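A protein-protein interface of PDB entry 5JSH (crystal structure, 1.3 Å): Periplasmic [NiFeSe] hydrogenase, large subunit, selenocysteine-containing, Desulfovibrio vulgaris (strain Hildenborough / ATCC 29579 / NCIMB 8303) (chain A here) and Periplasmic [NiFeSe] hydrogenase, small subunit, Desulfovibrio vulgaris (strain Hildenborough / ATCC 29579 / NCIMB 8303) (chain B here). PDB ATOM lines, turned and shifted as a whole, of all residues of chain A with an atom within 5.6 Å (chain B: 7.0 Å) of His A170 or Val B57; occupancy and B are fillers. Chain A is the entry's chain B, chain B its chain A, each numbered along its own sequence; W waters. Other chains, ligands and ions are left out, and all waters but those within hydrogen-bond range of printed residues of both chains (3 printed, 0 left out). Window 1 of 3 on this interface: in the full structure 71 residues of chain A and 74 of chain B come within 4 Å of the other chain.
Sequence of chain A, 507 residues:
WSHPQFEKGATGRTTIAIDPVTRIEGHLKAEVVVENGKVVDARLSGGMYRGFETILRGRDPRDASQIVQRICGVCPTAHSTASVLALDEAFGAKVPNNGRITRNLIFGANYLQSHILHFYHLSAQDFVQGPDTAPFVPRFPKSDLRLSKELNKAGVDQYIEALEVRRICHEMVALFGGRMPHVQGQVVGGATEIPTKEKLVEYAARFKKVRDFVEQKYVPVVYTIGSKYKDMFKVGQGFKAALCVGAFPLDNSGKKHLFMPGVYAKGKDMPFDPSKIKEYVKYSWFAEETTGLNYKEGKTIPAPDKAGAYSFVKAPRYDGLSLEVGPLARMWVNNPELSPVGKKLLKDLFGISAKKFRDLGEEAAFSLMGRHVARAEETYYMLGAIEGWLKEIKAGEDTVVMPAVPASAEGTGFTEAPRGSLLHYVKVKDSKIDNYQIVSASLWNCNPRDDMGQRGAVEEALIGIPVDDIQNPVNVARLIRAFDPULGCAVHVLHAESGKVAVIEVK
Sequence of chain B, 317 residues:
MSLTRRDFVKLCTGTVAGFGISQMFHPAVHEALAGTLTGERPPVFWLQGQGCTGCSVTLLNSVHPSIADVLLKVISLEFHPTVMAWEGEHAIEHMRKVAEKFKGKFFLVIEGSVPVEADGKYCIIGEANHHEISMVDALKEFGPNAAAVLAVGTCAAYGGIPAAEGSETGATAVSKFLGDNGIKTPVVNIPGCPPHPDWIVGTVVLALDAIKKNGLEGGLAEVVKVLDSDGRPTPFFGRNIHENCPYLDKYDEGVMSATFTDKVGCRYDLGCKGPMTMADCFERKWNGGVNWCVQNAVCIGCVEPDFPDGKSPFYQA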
ATOM      1  N   GLY A  73      -8.037  10.289  20.787  1.00  0.00           N
ATOM      2  CA  GLY A  73      -9.188  11.064  21.219  1.00  0.00           C
ATOM      3  C   GLY A  73      -9.691  10.808  22.623  1.00  0.00           C
ATOM      4  O   GLY A  73     -10.623  11.488  23.072  1.00  0.00           O
ATOM      5  N   VAL A  74      -9.107   9.816  23.295  1.00  0.00           N
ATOM      6  CA  VAL A  74      -9.385   9.566  24.708  1.00  0.00           C
ATOM      7  C   VAL A  74      -8.471  10.406  25.593  1.00  0.00           C
ATOM      8  O   VAL A  74      -8.925  10.970  26.589  1.00  0.00           O
ATOM      9  CB  VAL A  74      -9.258   8.057  25.031  1.00  0.00           C
ATOM     10  CG1 VAL A  74      -9.503   7.801  26.516  1.00  0.00           C
ATOM     11  CG2 VAL A  74     -10.215   7.230  24.183  1.00  0.00           C
ATOM     12  N   ALA A 109      -9.177  17.766  34.506  1.00  0.00           N
ATOM     13  CA  ALA A 109     -10.552  17.342  34.264  1.00  0.00           C
ATOM     14  C   ALA A 109     -10.617  16.100  33.383  1.00  0.00           C
ATOM     15  O   ALA A 109     -11.516  15.271  33.556  1.00  0.00           O
ATOM     16  CB  ALA A 109     -11.365  18.487  33.663  1.00  0.00           C
ATOM     17  N   ASN A 110      -9.686  15.947  32.437  1.00  0.00           N
ATOM     18  CA  ASN A 110      -9.698  14.735  31.634  1.00  0.00           C
ATOM     19  C   ASN A 110      -9.136  13.520  32.355  1.00  0.00           C
ATOM     20  O   ASN A 110      -9.478  12.408  31.962  1.00  0.00           O
ATOM     21  CB  ASN A 110      -9.011  14.866  30.278  1.00  0.00           C
ATOM     22  CG  ASN A 110      -9.528  13.829  29.300  1.00  0.00           C
ATOM     23  OD1 ASN A 110     -10.742  13.689  29.121  1.00  0.00           O
ATOM     24  ND2 ASN A 110      -8.629  13.097  28.664  1.00  0.00           N
ATOM     25  N   GLN A 113     -12.320  12.223  33.639  1.00  0.00           N
ATOM     26  CA  GLN A 113     -13.089  11.603  32.565  1.00  0.00           C
ATOM     27  C   GLN A 113     -12.529  10.239  32.202  1.00  0.00           C
ATOM     28  O   GLN A 113     -13.278   9.279  31.980  1.00  0.00           O
ATOM     29  CB  GLN A 113     -13.042  12.473  31.308  1.00  0.00           C
ATOM     30  CG  GLN A 113     -13.924  11.929  30.170  1.00  0.00           C
ATOM     31  CD  GLN A 113     -13.261  10.958  29.182  1.00  0.00           C
ATOM     32  OE1 GLN A 113     -13.975  10.143  28.580  1.00  0.00           O
ATOM     33  NE2 GLN A 113     -11.948  11.066  28.960  1.00  0.00           N
ATOM     34  N   LEU A 117     -14.288   6.630  32.569  1.00  0.00           N
ATOM     35  CA  LEU A 117     -14.541   5.892  31.337  1.00  0.00           C
ATOM     36  C   LEU A 117     -13.915   4.510  31.414  1.00  0.00           C
ATOM     37  O   LEU A 117     -14.537   3.504  31.046  1.00  0.00           O
ATOM     38  CB  LEU A 117     -13.942   6.653  30.152  1.00  0.00           C
ATOM     39  CG  LEU A 117     -13.964   5.975  28.782  1.00  0.00           C
ATOM     40  CD1 LEU A 117     -15.355   6.073  28.162  1.00  0.00           C
ATOM     41  CD2 LEU A 117     -12.885   6.568  27.857  1.00  0.00           C
ATOM     42  N   VAL A 165     -21.638  11.401  34.124  1.00  0.00           N
ATOM     43  CA  VAL A 165     -20.516  12.001  34.846  1.00  0.00           C
ATOM     44  C   VAL A 165     -19.323  12.242  33.920  1.00  0.00           C
ATOM     45  O   VAL A 165     -18.693  13.307  33.974  1.00  0.00           O
ATOM     46  CB  VAL A 165     -20.157  11.151  36.076  1.00  0.00           C
ATOM     47  CG1 VAL A 165     -18.952  11.733  36.792  1.00  0.00           C
ATOM     48  CG2 VAL A 165     -21.341  11.071  37.038  1.00  0.00           C
ATOM     49  N   ARG A 166     -18.972  11.265  33.065  1.00  0.00           N
ATOM     50  CA  ARG A 166     -17.830  11.484  32.174  1.00  0.00           C
ATOM     51  C   ARG A 166     -18.105  12.593  31.170  1.00  0.00           C
ATOM     52  O   ARG A 166     -17.179  13.315  30.776  1.00  0.00           O
ATOM     53  CB  ARG A 166     -17.356  10.198  31.471  1.00  0.00           C
ATOM     54  CG  ARG A 166     -18.355   9.546  30.517  1.00  0.00           C
ATOM     55  CD  ARG A 166     -17.683   8.842  29.329  1.00  0.00           C
ATOM     56  NE  ARG A 166     -16.819   9.759  28.593  1.00  0.00           N
ATOM     57  CZ  ARG A 166     -17.240  10.777  27.848  1.00  0.00           C
ATOM     58  NH1 ARG A 166     -18.537  11.010  27.691  1.00  0.00           N
ATOM     59  NH2 ARG A 166     -16.343  11.587  27.272  1.00  0.00           N
ATOM     60  N   ARG A 167     -19.367  12.741  30.745  1.00  0.00           N
ATOM     61  CA  ARG A 167     -19.723  13.837  29.854  1.00  0.00           C
ATOM     62  C   ARG A 167     -19.536  15.182  30.550  1.00  0.00           C
ATOM     63  O   ARG A 167     -19.033  16.143  29.948  1.00  0.00           O
ATOM     64  CB  ARG A 167     -21.162  13.650  29.364  1.00  0.00           C
ATOM     65  CG  ARG A 167     -21.661  14.773  28.450  1.00  0.00           C
ATOM     66  CD  ARG A 167     -23.103  14.578  28.003  1.00  0.00           C
ATOM     67  NE  ARG A 167     -24.026  14.508  29.133  1.00  0.00           N
ATOM     68  CZ  ARG A 167     -24.392  15.552  29.870  1.00  0.00           C
ATOM     69  NH1 ARG A 167     -23.899  16.762  29.613  1.00  0.00           N
ATOM     70  NH2 ARG A 167     -25.256  15.383  30.867  1.00  0.00           N
ATOM     71  N   ILE A 168     -19.943  15.269  31.819  1.00  0.00           N
ATOM     72  CA  ILE A 168     -19.740  16.479  32.617  1.00  0.00           C
ATOM     73  C   ILE A 168     -18.255  16.805  32.751  1.00  0.00           C
ATOM     74  O   ILE A 168     -17.851  17.975  32.735  1.00  0.00           O
ATOM     75  CB  ILE A 168     -20.440  16.330  33.985  1.00  0.00           C
ATOM     76  CG1 ILE A 168     -21.951  16.348  33.799  1.00  0.00           C
ATOM     77  CG2 ILE A 168     -20.001  17.428  34.950  1.00  0.00           C
ATOM     78  CD1 ILE A 168     -22.706  15.916  35.041  1.00  0.00           C
ATOM     79  N   CYS A 169     -17.414  15.780  32.892  1.00  0.00           N
ATOM     80  CA  CYS A 169     -15.977  16.011  32.930  1.00  0.00           C
ATOM     81  C   CYS A 169     -15.486  16.687  31.651  1.00  0.00           C
ATOM     82  O   CYS A 169     -14.621  17.566  31.702  1.00  0.00           O
ATOM     83  CB  CYS A 169     -15.236  14.694  33.131  1.00  0.00           C
ATOM     84  SG  CYS A 169     -15.382  13.932  34.771  1.00  0.00           S
ATOM     85  N   HIS A 170     -16.014  16.286  30.494  1.00  0.00           N
ATOM     86  CA  HIS A 170     -15.637  16.958  29.250  1.00  0.00           C
ATOM     87  C   HIS A 170     -16.175  18.383  29.165  1.00  0.00           C
ATOM     88  O   HIS A 170     -15.525  19.235  28.550  1.00  0.00           O
ATOM     89  CB  HIS A 170     -16.005  16.106  28.044  1.00  0.00           C
ATOM     90  CG  HIS A 170     -14.917  15.151  27.663  1.00  0.00           C
ATOM     91  ND1 HIS A 170     -14.968  14.371  26.533  1.00  0.00           N
ATOM     92  CD2 HIS A 170     -13.737  14.872  28.263  1.00  0.00           C
ATOM     93  CE1 HIS A 170     -13.857  13.660  26.443  1.00  0.00           C
ATOM     94  NE2 HIS A 170     -13.092  13.951  27.479  1.00  0.00           N
ATOM     95  N   GLU A 171     -17.338  18.672  29.771  1.00  0.00           N
ATOM     96  CA  GLU A 171     -17.755  20.066  29.896  1.00  0.00           C
ATOM     97  C   GLU A 171     -16.736  20.860  30.706  1.00  0.00           C
ATOM     98  O   GLU A 171     -16.398  21.996  30.352  1.00  0.00           O
ATOM     99  CB  GLU A 171     -19.146  20.172  30.525  1.00  0.00           C
ATOM    100  CG  GLU A 171     -20.255  19.548  29.681  1.00  0.00           C
ATOM    101  CD  GLU A 171     -21.645  19.804  30.234  1.00  0.00           C
ATOM    102  OE1 GLU A 171     -21.769  20.284  31.369  1.00  0.00           O
ATOM    103  OE2 GLU A 171     -22.625  19.509  29.524  1.00  0.00           O
ATOM    104  N   MET A 172     -16.221  20.271  31.791  1.00  0.00           N
ATOM    105  CA  MET A 172     -15.165  20.925  32.563  1.00  0.00           C
ATOM    106  C   MET A 172     -13.936  21.212  31.704  1.00  0.00           C
ATOM    107  O   MET A 172     -13.366  22.307  31.786  1.00  0.00           O
ATOM    108  CB  MET A 172     -14.803  20.083  33.789  1.00  0.00           C
ATOM    109  CG  MET A 172     -15.885  20.036  34.872  1.00  0.00           C
ATOM    110  SD  MET A 172     -15.636  18.704  36.050  1.00  0.00           S
ATOM    111  CE  MET A 172     -14.049  19.182  36.738  1.00  0.00           C
ATOM    112  N   VAL A 173     -13.499  20.231  30.895  1.00  0.00           N
ATOM    113  CA  VAL A 173     -12.353  20.434  30.007  1.00  0.00           C
ATOM    114  C   VAL A 173     -12.622  21.602  29.063  1.00  0.00           C
ATOM    115  O   VAL A 173     -11.753  22.467  28.827  1.00  0.00           O
ATOM    116  CB  VAL A 173     -12.030  19.151  29.212  1.00  0.00           C
ATOM    117  CG1 VAL A 173     -10.936  19.422  28.201  1.00  0.00           C
ATOM    118  CG2 VAL A 173     -11.628  18.015  30.137  1.00  0.00           C
ATOM    119  N   ALA A 174     -13.818  21.612  28.469  1.00  0.00           N
ATOM    120  CA  ALA A 174     -14.138  22.580  27.427  1.00  0.00           C
ATOM    121  C   ALA A 174     -14.302  23.998  27.962  1.00  0.00           C
ATOM    122  O   ALA A 174     -14.153  24.954  27.194  1.00  0.00           O
ATOM    123  CB  ALA A 174     -15.408  22.142  26.701  1.00  0.00           C
ATOM    124  N   LEU A 175     -14.612  24.163  29.249  1.00  0.00           N
ATOM    125  CA  LEU A 175     -14.815  25.511  29.778  1.00  0.00           C
ATOM    126  C   LEU A 175     -13.627  26.423  29.475  1.00  0.00           C
ATOM    127  O   LEU A 175     -13.811  27.554  29.020  1.00  0.00           O
ATOM    128  CB  LEU A 175     -15.144  25.470  31.276  1.00  0.00           C
ATOM    129  CG  LEU A 175     -16.616  25.207  31.600  1.00  0.00           C
ATOM    130  CD1 LEU A 175     -16.816  24.804  33.043  1.00  0.00           C
ATOM    131  CD2 LEU A 175     -17.466  26.438  31.279  1.00  0.00           C
ATOM    132  N   MET A 180     -13.919  19.378  23.503  1.00  0.00           N
ATOM    133  CA  MET A 180     -13.284  18.102  23.818  1.00  0.00           C
ATOM    134  C   MET A 180     -14.128  16.990  23.193  1.00  0.00           C
ATOM    135  O   MET A 180     -15.345  17.046  23.292  1.00  0.00           O
ATOM    136  CB  MET A 180     -13.192  17.949  25.339  1.00  0.00           C
ATOM    137  CG  MET A 180     -12.366  16.788  25.808  1.00  0.00           C
ATOM    138  SD  MET A 180     -10.593  16.936  25.407  1.00  0.00           S
ATOM    139  CE  MET A 180      -9.986  15.624  26.486  1.00  0.00           C
ATOM    140  N   PRO A 181     -13.499  15.987  22.546  1.00  0.00           N
ATOM    141  CA  PRO A 181     -12.073  15.824  22.236  1.00  0.00           C
ATOM    142  C   PRO A 181     -11.454  16.961  21.431  1.00  0.00           C
ATOM    143  O   PRO A 181     -12.140  17.683  20.708  1.00  0.00           O
ATOM    144  CB  PRO A 181     -12.037  14.545  21.392  1.00  0.00           C
ATOM    145  CG  PRO A 181     -13.241  13.785  21.794  1.00  0.00           C
ATOM    146  CD  PRO A 181     -14.287  14.851  22.032  1.00  0.00           C
ATOM    147  N   TRP B  46     -19.856  -0.674  13.891  1.00  0.00           N
ATOM    148  CA  TRP B  46     -18.937   0.463  13.954  1.00  0.00           C
ATOM    149  C   TRP B  46     -17.518  -0.063  13.781  1.00  0.00           C
ATOM    150  O   TRP B  46     -17.000  -0.758  14.668  1.00  0.00           O
ATOM    151  CB  TRP B  46     -19.099   1.175  15.293  1.00  0.00           C
ATOM    152  CG  TRP B  46     -18.376   2.485  15.426  1.00  0.00           C
ATOM    153  CD1 TRP B  46     -17.031   2.693  15.383  1.00  0.00           C
ATOM    154  CD2 TRP B  46     -18.972   3.762  15.673  1.00  0.00           C
ATOM    155  NE1 TRP B  46     -16.752   4.026  15.567  1.00  0.00           N
ATOM    156  CE2 TRP B  46     -17.927   4.701  15.766  1.00  0.00           C
ATOM    157  CE3 TRP B  46     -20.288   4.202  15.834  1.00  0.00           C
ATOM    158  CZ2 TRP B  46     -18.163   6.061  15.984  1.00  0.00           C
ATOM    159  CZ3 TRP B  46     -20.517   5.550  16.061  1.00  0.00           C
ATOM    160  CH2 TRP B  46     -19.462   6.456  16.139  1.00  0.00           C
ATOM    161  N   CYS B  52      -8.650   7.715  15.817  1.00  0.00           N
ATOM    162  CA  CYS B  52      -8.115   7.988  17.148  1.00  0.00           C
ATOM    163  C   CYS B  52      -9.122   7.709  18.259  1.00  0.00           C
ATOM    164  O   CYS B  52      -8.837   7.982  19.424  1.00  0.00           O
ATOM    165  CB  CYS B  52      -7.616   9.439  17.256  1.00  0.00           C
ATOM    166  SG  CYS B  52      -8.917  10.686  17.527  1.00  0.00           S
ATOM    167  N   THR B  53     -10.307   7.215  17.918  1.00  0.00           N
ATOM    168  CA  THR B  53     -11.411   6.934  18.831  1.00  0.00           C
ATOM    169  C   THR B  53     -12.113   8.231  19.252  1.00  0.00           C
ATOM    170  O   THR B  53     -13.086   8.196  20.022  1.00  0.00           O
ATOM    171  CB  THR B  53     -10.972   6.001  19.977  1.00  0.00           C
ATOM    172  OG1 THR B  53     -10.375   4.843  19.370  1.00  0.00           O
ATOM    173  CG2 THR B  53     -12.132   5.533  20.851  1.00  0.00           C
ATOM    174  N   GLY B  54     -11.684   9.380  18.734  1.00  0.00           N
ATOM    175  CA  GLY B  54     -12.330  10.627  19.084  1.00  0.00           C
ATOM    176  C   GLY B  54     -13.745  10.743  18.564  1.00  0.00           C
ATOM    177  O   GLY B  54     -14.563  11.457  19.156  1.00  0.00           O
ATOM    178  N   CYS B  55     -14.048  10.057  17.469  1.00  0.00           N
ATOM    179  CA  CYS B  55     -15.397  10.090  16.929  1.00  0.00           C
ATOM    180  C   CYS B  55     -16.358   9.256  17.786  1.00  0.00           C
ATOM    181  O   CYS B  55     -17.530   9.617  17.927  1.00  0.00           O
ATOM    182  CB  CYS B  55     -15.357   9.706  15.440  1.00  0.00           C
ATOM    183  SG  CYS B  55     -14.541  10.966  14.345  1.00  0.00           S
ATOM    184  N   SER B  56     -15.867   8.184  18.430  1.00  0.00           N
ATOM    185  CA  SER B  56     -16.648   7.459  19.427  1.00  0.00           C
ATOM    186  C   SER B  56     -16.824   8.296  20.684  1.00  0.00           C
ATOM    187  O   SER B  56     -17.924   8.373  21.243  1.00  0.00           O
ATOM    188  CB  SER B  56     -15.955   6.138  19.773  1.00  0.00           C
ATOM    189  OG  SER B  56     -16.035   5.199  18.713  1.00  0.00           O
ATOM    190  N   VAL B  57     -15.741   8.921  21.158  1.00  0.00           N
ATOM    191  CA  VAL B  57     -15.810   9.700  22.389  1.00  0.00           C
ATOM    192  C   VAL B  57     -16.751  10.889  22.231  1.00  0.00           C
ATOM    193  O   VAL B  57     -17.536  11.199  23.139  1.00  0.00           O
ATOM    194  CB  VAL B  57     -14.409  10.141  22.849  1.00  0.00           C
ATOM    195  CG1 VAL B  57     -14.510  11.077  24.040  1.00  0.00           C
ATOM    196  CG2 VAL B  57     -13.572   8.938  23.204  1.00  0.00           C
ATOM    197  N   THR B  58     -16.695  11.578  21.088  1.00  0.00           N
ATOM    198  CA  THR B  58     -17.593  12.715  20.908  1.00  0.00           C
ATOM    199  C   THR B  58     -19.056  12.264  20.975  1.00  0.00           C
ATOM    200  O   THR B  58     -19.906  12.958  21.547  1.00  0.00           O
ATOM    201  CB  THR B  58     -17.248  13.472  19.625  1.00  0.00           C
ATOM    202  OG1 THR B  58     -17.689  14.833  19.764  1.00  0.00           O
ATOM    203  CG2 THR B  58     -17.877  12.856  18.377  1.00  0.00           C
ATOM    204  N   LEU B  59     -19.352  11.081  20.426  1.00  0.00           N
ATOM    205  CA  LEU B  59     -20.709  10.545  20.475  1.00  0.00           C
ATOM    206  C   LEU B  59     -21.140  10.292  21.909  1.00  0.00           C
ATOM    207  O   LEU B  59     -22.285  10.563  22.279  1.00  0.00           O
ATOM    208  CB  LEU B  59     -20.790   9.262  19.656  1.00  0.00           C
ATOM    209  CG  LEU B  59     -22.121   8.519  19.667  1.00  0.00           C
ATOM    210  CD1 LEU B  59     -23.258   9.424  19.218  1.00  0.00           C
ATOM    211  CD2 LEU B  59     -22.019   7.278  18.785  1.00  0.00           C
ATOM    212  N   LEU B  60     -20.225   9.784  22.741  1.00  0.00           N
ATOM    213  CA  LEU B  60     -20.540   9.580  24.148  1.00  0.00           C
ATOM    214  C   LEU B  60     -20.956  10.880  24.834  1.00  0.00           C
ATOM    215  O   LEU B  60     -21.625  10.831  25.877  1.00  0.00           O
ATOM    216  CB  LEU B  60     -19.320   9.008  24.871  1.00  0.00           C
ATOM    217  CG  LEU B  60     -18.827   7.626  24.413  1.00  0.00           C
ATOM    218  CD1 LEU B  60     -17.657   7.205  25.273  1.00  0.00           C
ATOM    219  CD2 LEU B  60     -19.934   6.598  24.471  1.00  0.00           C
ATOM    220  N   ASN B  61     -20.590  12.037  24.268  1.00  0.00           N
ATOM    221  CA  ASN B  61     -20.919  13.336  24.854  1.00  0.00           C
ATOM    222  C   ASN B  61     -22.283  13.871  24.430  1.00  0.00           C
ATOM    223  O   ASN B  61     -22.618  15.005  24.782  1.00  0.00           O
ATOM    224  CB  ASN B  61     -19.840  14.370  24.524  1.00  0.00           C
ATOM    225  CG  ASN B  61     -18.558  14.132  25.275  1.00  0.00           C
ATOM    226  OD1 ASN B  61     -18.528  13.495  26.351  1.00  0.00           O
ATOM    227  ND2 ASN B  61     -17.478  14.652  24.722  1.00  0.00           N
ATOM    228  N   SER B  62     -23.075  13.111  23.676  1.00  0.00           N
ATOM    229  CA  SER B  62     -24.385  13.594  23.243  1.00  0.00           C
ATOM    230  C   SER B  62     -25.273  13.958  24.441  1.00  0.00           C
ATOM    231  O   SER B  62     -25.394  13.207  25.405  1.00  0.00           O
ATOM    232  CB  SER B  62     -25.062  12.508  22.405  1.00  0.00           C
ATOM    233  OG  SER B  62     -26.286  12.988  21.866  1.00  0.00           O
ATOM    234  N   HIS B  80     -18.844  -2.921  18.122  1.00  0.00           N
ATOM    235  CA  HIS B  80     -18.088  -1.698  18.356  1.00  0.00           C
ATOM    236  C   HIS B  80     -16.938  -2.105  19.258  1.00  0.00           C
ATOM    237  O   HIS B  80     -17.173  -2.447  20.418  1.00  0.00           O
ATOM    238  CB  HIS B  80     -18.925  -0.627  19.045  1.00  0.00           C
ATOM    239  CG  HIS B  80     -18.233   0.697  19.088  1.00  0.00           C
ATOM    240  ND1 HIS B  80     -16.967   0.852  19.611  1.00  0.00           N
ATOM    241  CD2 HIS B  80     -18.608   1.922  18.636  1.00  0.00           C
ATOM    242  CE1 HIS B  80     -16.585   2.111  19.466  1.00  0.00           C
ATOM    243  NE2 HIS B  80     -17.578   2.784  18.907  1.00  0.00           N
ATOM    244  N   THR B  82     -14.639  -0.687  21.007  1.00  0.00           N
ATOM    245  CA  THR B  82     -14.311   0.031  22.230  1.00  0.00           C
ATOM    246  C   THR B  82     -15.247  -0.304  23.387  1.00  0.00           C
ATOM    247  O   THR B  82     -14.835  -0.196  24.544  1.00  0.00           O
ATOM    248  CB  THR B  82     -14.347   1.549  21.975  1.00  0.00           C
ATOM    249  OG1 THR B  82     -13.678   1.848  20.748  1.00  0.00           O
ATOM    250  CG2 THR B  82     -13.685   2.318  23.086  1.00  0.00           C
ATOM    251  N   GLU B 111     -15.037   4.877  11.223  1.00  0.00           N
ATOM    252  CA  GLU B 111     -14.257   5.879  11.955  1.00  0.00           C
ATOM    253  C   GLU B 111     -12.796   5.669  11.571  1.00  0.00           C
ATOM    254  O   GLU B 111     -12.265   4.576  11.790  1.00  0.00           O
ATOM    255  CB  GLU B 111     -14.449   5.683  13.475  1.00  0.00           C
ATOM    256  CG  GLU B 111     -13.474   6.474  14.405  1.00  0.00           C
ATOM    257  CD  GLU B 111     -13.828   6.420  15.907  1.00  0.00           C
ATOM    258  OE1 GLU B 111     -14.472   5.442  16.361  1.00  0.00           O
ATOM    259  OE2 GLU B 111     -13.408   7.348  16.656  1.00  0.00           O
ATOM    260  N   PRO B 194     -12.999  16.164  16.220  1.00  0.00           N
ATOM    261  CA  PRO B 194     -14.106  15.272  15.866  1.00  0.00           C
ATOM    262  C   PRO B 194     -15.361  16.029  15.434  1.00  0.00           C
ATOM    263  O   PRO B 194     -15.464  17.250  15.642  1.00  0.00           O
ATOM    264  CB  PRO B 194     -14.437  14.594  17.199  1.00  0.00           C
ATOM    265  CG  PRO B 194     -14.200  15.692  18.207  1.00  0.00           C
ATOM    266  CD  PRO B 194     -13.036  16.524  17.652  1.00  0.00           C
ATOM    267  N   PRO B 197     -21.343  15.660  18.558  1.00  0.00           N
ATOM    268  CA  PRO B 197     -22.304  14.546  18.677  1.00  0.00           C
ATOM    269  C   PRO B 197     -23.617  14.813  17.981  1.00  0.00           C
ATOM    270  O   PRO B 197     -24.213  13.890  17.436  1.00  0.00           O
ATOM    271  CB  PRO B 197     -22.492  14.378  20.194  1.00  0.00           C
ATOM    272  CG  PRO B 197     -21.984  15.658  20.796  1.00  0.00           C
ATOM    273  CD  PRO B 197     -20.882  16.112  19.879  1.00  0.00           C
ATOM    274  N   ASN B 287     -19.811  20.792  23.790  1.00  0.00           N
ATOM    275  CA  ASN B 287     -19.803  20.228  25.138  1.00  0.00           C
ATOM    276  C   ASN B 287     -20.861  20.877  26.030  1.00  0.00           C
ATOM    277  O   ASN B 287     -20.563  21.461  27.071  1.00  0.00           O
ATOM    278  CB  ASN B 287     -18.401  20.325  25.742  1.00  0.00           C
ATOM    279  CG  ASN B 287     -17.381  19.563  24.924  1.00  0.00           C
ATOM    280  OD1 ASN B 287     -16.694  20.117  24.061  1.00  0.00           O
ATOM    281  ND2 ASN B 287     -17.308  18.264  25.164  1.00  0.00           N
ATOM    282  N   VAL B 290     -20.872  25.034  26.450  1.00  0.00           N
ATOM    283  CA  VAL B 290     -20.022  25.799  27.364  1.00  0.00           C
ATOM    284  C   VAL B 290     -18.941  26.622  26.665  1.00  0.00           C
ATOM    285  O   VAL B 290     -18.370  27.520  27.297  1.00  0.00           O
ATOM    286  CB  VAL B 290     -19.387  24.911  28.453  1.00  0.00           C
ATOM    287  CG1 VAL B 290     -20.466  24.226  29.290  1.00  0.00           C
ATOM    288  CG2 VAL B 290     -18.406  23.896  27.855  1.00  0.00           C
HETATM  289  O   HOH W   1     -17.817  16.267  22.156  1.00  0.00           O
HETATM  290  O   HOH W   2     -20.831   9.373  28.158  1.00  0.00           O
HETATM  291  O   HOH W   3     -19.208  17.111  27.124  1.00  0.00           O
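Water W1 lies within hydrogen-bond range of the side-chain hydroxyl (OG1) of Thr B58 (2.8 Å), the backbone carbonyl oxygen (O) of Met A180 (2.8 Å) and the side-chain amide nitrogen (ND2) of Asn B61 (3.1 Å). Water W2 bridges O of Leu B60 (2.8 Å) and NH1 of Arg A166 (2.9 Å). Water W3 bridges the side-chain amide nitrogen (ND2) of Asn B287 (3.0 Å) and the backbone carbonyl oxygen (O) of Arg A167 (3.0 Å).
CA of Gly A73 touches CA of Gly B54, 3.8 Å away. Leu A117 touches Leu B60. Arg A166 touches Leu B60 (NH1 to CB, 3.5 Å). His A170 touches Val B57 (CE1 to CG1, 3.6 Å). Asn B287 touches His A170 (ND2 to CB, 3.8 Å). Asn B287 touches Glu A171 (O to CG, 3.3 Å). Val B290 touches Ala A174 (CG2 to CB, 3.7 Å). Asn B61 touches Met A180. Gly B54 touches Pro A181. Pro A181 touches Val B57.
Printed residues of chain B within 4 Å of His A170: Val B57 (3.6 Å), Asn B61 (3.1 Å) and Asn B287 (3.8 Å). Of chain A, only Gly A73 (3.9 Å), Val A74 (3.9 Å), Arg A166 (3.8 Å), His A170 (3.6 Å) and Pro A181 (3.7 Å) come within 4 Å of Val B57. Printed residues of chain B within 4 Å of Gly A73: Cys B52 (2.8 Å), Gly B54 (3.8 Å) and Val B57 (3.9 Å). Of the printed residues of chain A, Cys B52 touches Gly A73 (2.8 Å). Leu B59 touches none of the printed residues of chain A. The nearest residue of chain B that does not touch His A170 is Val B290 (5.5 Å).
The backbone carbonyl oxygen (O) of Cys B52 is in hydrogen-bond range of the backbone NH (N) of Gly A73 (2.8 Å). N of Met A180 is in hydrogen-bond range of OD1 of Asn B287 (2.9 Å). The guanidinium group (NH1) of Arg A166 is in hydrogen-bond range of the side-chain amide oxygen (OD1) of Asn B61 (2.8 Å). A ring nitrogen (ND1) of His A170 is in hydrogen-bond range of the side-chain amide nitrogen (ND2) of Asn B61, 3.1 Å away.
Hydrophobic or aromatic side chains of chain A that line the printed part of chain B: Val A74, Leu A117, His A170, Ala A174, Leu A175 and Pro A181. Of the 19 printed residues of chain B, 9 touch a printed residue of chain A. Hydrophobic or aromatic side chains of chain B within 4 Å of the printed part of chain A: Val B57, Leu B60, Pro B194 and Val B290. Among the printed residues, no Asp or Glu carboxylate lies within 4 Å of a Lys or Arg side-chain nitrogen of the other chain.
The backbone NH (N) of Gly B54 lies within hydrogen-bond range of the side-chain carboxylate (OE2) of Glu B111. The side-chain amide nitrogen (ND2) of Asn A110 is in hydrogen-bond range of the backbone carbonyl oxygen (O) of Val A74 (3.0 Å). The side-chain sulfur (SG) of Cys B52 lies close to the backbone NH (N) of Gly B54, at 3.3 Å.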
